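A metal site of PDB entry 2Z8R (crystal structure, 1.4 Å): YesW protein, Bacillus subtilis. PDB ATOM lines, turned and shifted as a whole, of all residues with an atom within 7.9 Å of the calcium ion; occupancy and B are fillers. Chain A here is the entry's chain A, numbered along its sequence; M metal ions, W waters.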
ATOM      1  N   ASP A 420      19.572  -4.871  -0.672  1.00  0.00           N
ATOM      2  CA  ASP A 420      20.045  -5.048  -2.039  1.00  0.00           C
ATOM      3  C   ASP A 420      18.937  -5.677  -2.866  1.00  0.00           C
ATOM      4  O   ASP A 420      18.700  -6.877  -2.786  1.00  0.00           O
ATOM      5  CB  ASP A 420      21.304  -5.911  -2.083  1.00  0.00           C
ATOM      6  CG  ASP A 420      21.915  -5.978  -3.469  1.00  0.00           C
ATOM      7  OD1 ASP A 420      21.427  -5.244  -4.349  1.00  0.00           O
ATOM      8  OD2 ASP A 420      22.906  -6.711  -3.665  1.00  0.00           O
ATOM      9  N   ILE A 456      14.056  -9.445   3.883  1.00  0.00           N
ATOM     10  CA  ILE A 456      14.226 -10.843   4.272  1.00  0.00           C
ATOM     11  C   ILE A 456      14.926 -11.618   3.163  1.00  0.00           C
ATOM     12  O   ILE A 456      14.590 -11.468   1.986  1.00  0.00           O
ATOM     13  CB  ILE A 456      12.876 -11.535   4.604  1.00  0.00           C
ATOM     14  CG1 ILE A 456      13.135 -12.963   5.113  1.00  0.00           C
ATOM     15  CG2 ILE A 456      11.902 -11.522   3.379  1.00  0.00           C
ATOM     16  CD1 ILE A 456      11.914 -13.653   5.663  1.00  0.00           C
ATOM     17  N   TRP A 457      15.909 -12.445   3.536  1.00  0.00           N
ATOM     18  CA  TRP A 457      16.492 -13.377   2.572  1.00  0.00           C
ATOM     19  C   TRP A 457      15.624 -14.619   2.522  1.00  0.00           C
ATOM     20  O   TRP A 457      15.641 -15.421   3.456  1.00  0.00           O
ATOM     21  CB  TRP A 457      17.950 -13.723   2.913  1.00  0.00           C
ATOM     22  CG  TRP A 457      18.866 -12.546   2.725  1.00  0.00           C
ATOM     23  CD1 TRP A 457      19.185 -11.937   1.537  1.00  0.00           C
ATOM     24  CD2 TRP A 457      19.550 -11.793   3.745  1.00  0.00           C
ATOM     25  NE1 TRP A 457      20.022 -10.873   1.753  1.00  0.00           N
ATOM     26  CE2 TRP A 457      20.262 -10.755   3.097  1.00  0.00           C
ATOM     27  CE3 TRP A 457      19.618 -11.888   5.147  1.00  0.00           C
ATOM     28  CZ2 TRP A 457      21.036  -9.829   3.792  1.00  0.00           C
ATOM     29  CZ3 TRP A 457      20.408 -10.962   5.848  1.00  0.00           C
ATOM     30  CH2 TRP A 457      21.103  -9.949   5.158  1.00  0.00           C
ATOM     31  N   TRP A 458      14.869 -14.764   1.419  1.00  0.00           N
ATOM     32  CA  TRP A 458      13.870 -15.829   1.312  1.00  0.00           C
ATOM     33  C   TRP A 458      14.111 -16.778   0.149  1.00  0.00           C
ATOM     34  O   TRP A 458      14.062 -17.993   0.323  1.00  0.00           O
ATOM     35  CB  TRP A 458      12.469 -15.233   1.212  1.00  0.00           C
ATOM     36  CG  TRP A 458      11.390 -16.272   1.200  1.00  0.00           C
ATOM     37  CD1 TRP A 458      10.594 -16.615   0.140  1.00  0.00           C
ATOM     38  CD2 TRP A 458      10.989 -17.100   2.298  1.00  0.00           C
ATOM     39  NE1 TRP A 458       9.714 -17.622   0.521  1.00  0.00           N
ATOM     40  CE2 TRP A 458       9.931 -17.931   1.833  1.00  0.00           C
ATOM     41  CE3 TRP A 458      11.413 -17.218   3.633  1.00  0.00           C
ATOM     42  CZ2 TRP A 458       9.297 -18.869   2.669  1.00  0.00           C
ATOM     43  CZ3 TRP A 458      10.775 -18.159   4.459  1.00  0.00           C
ATOM     44  CH2 TRP A 458       9.727 -18.970   3.965  1.00  0.00           C
ATOM     45  N   ASP A 459      14.353 -16.231  -1.040  1.00  0.00           N
ATOM     46  CA  ASP A 459      14.555 -17.072  -2.219  1.00  0.00           C
ATOM     47  C   ASP A 459      16.020 -17.489  -2.328  1.00  0.00           C
ATOM     48  O   ASP A 459      16.779 -17.355  -1.364  1.00  0.00           O
ATOM     49  CB  ASP A 459      13.999 -16.419  -3.500  1.00  0.00           C
ATOM     50  CG  ASP A 459      14.776 -15.199  -3.936  1.00  0.00           C
ATOM     51  OD1 ASP A 459      15.944 -15.047  -3.523  1.00  0.00           O
ATOM     52  OD2 ASP A 459      14.186 -14.406  -4.711  1.00  0.00           O
ATOM     53  N   GLY A 460      16.416 -18.022  -3.489  1.00  0.00           N
ATOM     54  CA  GLY A 460      17.746 -18.586  -3.656  1.00  0.00           C
ATOM     55  C   GLY A 460      18.817 -17.593  -4.063  1.00  0.00           C
ATOM     56  O   GLY A 460      19.999 -17.929  -4.036  1.00  0.00           O
ATOM     57  N   ASP A 461      18.435 -16.377  -4.443  1.00  0.00           N
ATOM     58  CA  ASP A 461      19.436 -15.401  -4.877  1.00  0.00           C
ATOM     59  C   ASP A 461      19.973 -14.535  -3.730  1.00  0.00           C
ATOM     60  O   ASP A 461      19.408 -14.496  -2.634  1.00  0.00           O
ATOM     61  CB  ASP A 461      18.976 -14.595  -6.111  1.00  0.00           C
ATOM     62  CG  ASP A 461      17.964 -13.495  -5.799  1.00  0.00           C
ATOM     63  OD1 ASP A 461      17.880 -13.022  -4.638  1.00  0.00           O
ATOM     64  OD2 ASP A 461      17.272 -13.052  -6.741  1.00  0.00           O
ATOM     65  N   LEU A 462      21.085 -13.854  -3.981  1.00  0.00           N
ATOM     66  CA  LEU A 462      21.742 -13.046  -2.956  1.00  0.00           C
ATOM     67  C   LEU A 462      21.085 -11.676  -2.745  1.00  0.00           C
ATOM     68  O   LEU A 462      21.421 -10.983  -1.790  1.00  0.00           O
ATOM     69  CB  LEU A 462      23.237 -12.891  -3.270  1.00  0.00           C
ATOM     70  CG  LEU A 462      24.008 -14.207  -3.218  1.00  0.00           C
ATOM     71  CD1 LEU A 462      25.409 -13.975  -3.749  1.00  0.00           C
ATOM     72  CD2 LEU A 462      24.049 -14.809  -1.814  1.00  0.00           C
ATOM     73  N   LEU A 463      20.151 -11.298  -3.613  1.00  0.00           N
ATOM     74  CA  LEU A 463      19.361 -10.098  -3.357  1.00  0.00           C
ATOM     75  C   LEU A 463      18.447 -10.350  -2.155  1.00  0.00           C
ATOM     76  O   LEU A 463      18.211 -11.509  -1.783  1.00  0.00           O
ATOM     77  CB  LEU A 463      18.547  -9.702  -4.594  1.00  0.00           C
ATOM     78  CG  LEU A 463      19.367  -9.461  -5.859  1.00  0.00           C
ATOM     79  CD1 LEU A 463      18.422  -9.272  -7.053  1.00  0.00           C
ATOM     80  CD2 LEU A 463      20.234  -8.220  -5.711  1.00  0.00           C
ATOM     81  N   ARG A 464      17.949  -9.287  -1.535  1.00  0.00           N
ATOM     82  CA  ARG A 464      17.048  -9.426  -0.400  1.00  0.00           C
ATOM     83  C   ARG A 464      15.608  -9.130  -0.810  1.00  0.00           C
ATOM     84  O   ARG A 464      15.342  -8.168  -1.530  1.00  0.00           O
ATOM     85  CB  ARG A 464      17.512  -8.542   0.766  1.00  0.00           C
ATOM     86  CG  ARG A 464      17.056  -9.054   2.124  1.00  0.00           C
ATOM     87  CD  ARG A 464      17.674  -8.290   3.271  1.00  0.00           C
ATOM     88  NE  ARG A 464      17.454  -9.036   4.517  1.00  0.00           N
ATOM     89  CZ  ARG A 464      17.758  -8.560   5.735  1.00  0.00           C
ATOM     90  NH1 ARG A 464      18.305  -7.357   5.878  1.00  0.00           N
ATOM     91  NH2 ARG A 464      17.540  -9.320   6.810  1.00  0.00           N
ATOM     92  N   GLU A 465      14.705  -9.989  -0.330  1.00  0.00           N
ATOM     93  CA  GLU A 465      13.282  -9.859  -0.593  1.00  0.00           C
ATOM     94  C   GLU A 465      12.656  -8.948   0.467  1.00  0.00           C
ATOM     95  O   GLU A 465      13.346  -8.471   1.374  1.00  0.00           O
ATOM     96  CB  GLU A 465      12.630 -11.248  -0.664  1.00  0.00           C
ATOM     97  CG  GLU A 465      13.054 -12.090  -1.893  1.00  0.00           C
ATOM     98  CD  GLU A 465      14.542 -12.464  -1.923  1.00  0.00           C
ATOM     99  OE1 GLU A 465      14.974 -13.281  -1.090  1.00  0.00           O
ATOM    100  OE2 GLU A 465      15.246 -11.957  -2.830  1.00  0.00           O
ATOM    101  N   LYS A 474       8.905  -9.879  -3.917  1.00  0.00           N
ATOM    102  CA  LYS A 474      10.189  -9.701  -4.591  1.00  0.00           C
ATOM    103  C   LYS A 474      10.116  -8.574  -5.613  1.00  0.00           C
ATOM    104  O   LYS A 474       9.214  -8.528  -6.447  1.00  0.00           O
ATOM    105  CB  LYS A 474      10.686 -10.995  -5.247  1.00  0.00           C
ATOM    106  CG  LYS A 474      12.134 -10.904  -5.691  1.00  0.00           C
ATOM    107  CD  LYS A 474      12.589 -12.155  -6.388  1.00  0.00           C
ATOM    108  CE  LYS A 474      14.038 -12.049  -6.837  1.00  0.00           C
ATOM    109  NZ  LYS A 474      15.003 -12.006  -5.700  1.00  0.00           N
ATOM    110  N   MET A 485       5.498 -13.181  -3.459  1.00  0.00           N
ATOM    111  CA  MET A 485       6.198 -14.465  -3.490  1.00  0.00           C
ATOM    112  C   MET A 485       5.588 -15.472  -2.504  1.00  0.00           C
ATOM    113  O   MET A 485       5.631 -16.680  -2.741  1.00  0.00           O
ATOM    114  CB  MET A 485       7.677 -14.232  -3.179  1.00  0.00           C
ATOM    115  CG  MET A 485       8.567 -15.454  -3.202  1.00  0.00           C
ATOM    116  SD  MET A 485      10.299 -14.968  -3.181  1.00  0.00           S
ATOM    117  CE  MET A 485      10.594 -14.738  -4.923  1.00  0.00           C
ATOM    118  N   TRP A 511      21.094 -20.571   5.308  1.00  0.00           N
ATOM    119  CA  TRP A 511      21.198 -19.144   5.602  1.00  0.00           C
ATOM    120  C   TRP A 511      19.955 -18.294   5.373  1.00  0.00           C
ATOM    121  O   TRP A 511      19.919 -17.171   5.858  1.00  0.00           O
ATOM    122  CB  TRP A 511      22.372 -18.543   4.831  1.00  0.00           C
ATOM    123  CG  TRP A 511      22.203 -18.593   3.337  1.00  0.00           C
ATOM    124  CD1 TRP A 511      22.478 -19.655   2.508  1.00  0.00           C
ATOM    125  CD2 TRP A 511      21.712 -17.542   2.483  1.00  0.00           C
ATOM    126  NE1 TRP A 511      22.213 -19.321   1.194  1.00  0.00           N
ATOM    127  CE2 TRP A 511      21.737 -18.037   1.152  1.00  0.00           C
ATOM    128  CE3 TRP A 511      21.292 -16.226   2.718  1.00  0.00           C
ATOM    129  CZ2 TRP A 511      21.322 -17.259   0.062  1.00  0.00           C
ATOM    130  CZ3 TRP A 511      20.883 -15.456   1.629  1.00  0.00           C
ATOM    131  CH2 TRP A 511      20.919 -15.968   0.320  1.00  0.00           C
ATOM    132  N   ARG A 512      18.962 -18.768   4.630  1.00  0.00           N
ATOM    133  CA  ARG A 512      17.753 -17.968   4.467  1.00  0.00           C
ATOM    134  C   ARG A 512      17.044 -17.787   5.813  1.00  0.00           C
ATOM    135  O   ARG A 512      17.239 -18.562   6.756  1.00  0.00           O
ATOM    136  CB  ARG A 512      16.812 -18.554   3.422  1.00  0.00           C
ATOM    137  CG  ARG A 512      17.145 -18.140   1.999  1.00  0.00           C
ATOM    138  CD  ARG A 512      18.336 -18.894   1.396  1.00  0.00           C
ATOM    139  NE  ARG A 512      18.147 -20.348   1.343  1.00  0.00           N
ATOM    140  CZ  ARG A 512      17.457 -20.978   0.390  1.00  0.00           C
ATOM    141  NH1 ARG A 512      16.843 -20.294  -0.566  1.00  0.00           N
ATOM    142  NH2 ARG A 512      17.352 -22.302   0.427  1.00  0.00           N
ATOM    143  N   THR A 534      18.788 -23.010  -3.339  1.00  0.00           N
ATOM    144  CA  THR A 534      19.848 -22.038  -3.563  1.00  0.00           C
ATOM    145  C   THR A 534      21.155 -22.749  -3.912  1.00  0.00           C
ATOM    146  O   THR A 534      21.386 -23.881  -3.482  1.00  0.00           O
ATOM    147  CB  THR A 534      20.070 -21.116  -2.328  1.00  0.00           C
ATOM    148  OG1 THR A 534      21.037 -20.116  -2.659  1.00  0.00           O
ATOM    149  CG2 THR A 534      20.561 -21.897  -1.100  1.00  0.00           C
ATOM    150  N   HIS A 536      23.901 -21.223  -3.044  1.00  0.00           N
ATOM    151  CA  HIS A 536      24.788 -20.551  -2.102  1.00  0.00           C
ATOM    152  C   HIS A 536      24.744 -21.132  -0.697  1.00  0.00           C
ATOM    153  O   HIS A 536      23.682 -21.466  -0.175  1.00  0.00           O
ATOM    154  CB  HIS A 536      24.474 -19.050  -2.038  1.00  0.00           C
ATOM    155  CG  HIS A 536      24.426 -18.389  -3.368  1.00  0.00           C
ATOM    156  ND1 HIS A 536      25.548 -18.226  -4.158  1.00  0.00           N
ATOM    157  CD2 HIS A 536      23.392 -17.833  -4.055  1.00  0.00           C
ATOM    158  CE1 HIS A 536      25.213 -17.601  -5.277  1.00  0.00           C
ATOM    159  NE2 HIS A 536      23.901 -17.355  -5.238  1.00  0.00           N
ATOM    160  N   LEU A 568      26.111  -8.716   2.346  1.00  0.00           N
ATOM    161  CA  LEU A 568      25.512  -9.912   1.784  1.00  0.00           C
ATOM    162  C   LEU A 568      24.630  -9.428   0.654  1.00  0.00           C
ATOM    163  O   LEU A 568      23.638  -8.748   0.897  1.00  0.00           O
ATOM    164  CB  LEU A 568      24.683 -10.645   2.845  1.00  0.00           C
ATOM    165  CG  LEU A 568      24.343 -12.120   2.609  1.00  0.00           C
ATOM    166  CD1 LEU A 568      23.680 -12.734   3.845  1.00  0.00           C
ATOM    167  CD2 LEU A 568      23.414 -12.288   1.406  1.00  0.00           C
HETATM  168 CA    CA M   1      17.139 -13.427  -2.411  1.00  0.00          CA
HETATM  169  O   HOH W   1      17.599 -14.882  -0.485  1.00  0.00           O
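OD2 of Asp 459 lies within salt-bridge range of NZ of Lys 474.
The side-chain carboxylate of Glu 465 lies close to the backbone NH of Trp 458.
The backbone carbonyl oxygen (O) of Asp 459 is in hydrogen-bond range of the guanidinium group (NH1) of Arg 512.
The side-chain carboxylate (OE2) of Glu 465 sits close to the side-chain amino group (NZ) of Lys 474 (2.9 Å).
The side-chain amino group (NZ) of Lys 474 lies within salt-bridge range of the side-chain carboxylate (OD2) of Asp 461.
The backbone carbonyl oxygen (O) of Ile 456 lies within hydrogen-bond range of the backbone NH (N) of Glu 465, at 2.8 Å.
Within 4 Å of the calcium ion: Asp 459, Asp 461, Leu 463 and Glu 465.
O of Leu 463 binds the calcium ion, at 2.3 Å.
OD1 of Asp 459 is bound to the calcium ion, 2.3 Å away.
OD1 of Asp 461 binds the calcium ion, at 2.4 Å.
OE2 of Glu 465 binds the calcium ion, 2.4 Å away.
Water W1 binds the calcium ion, 2.5 Å away.
The backbone carbonyl oxygen (O) of Asp 461 is bound to the calcium ion (2.5 Å).
The calcium ion is bound by OE1 of Glu 465 (2.5 Å).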
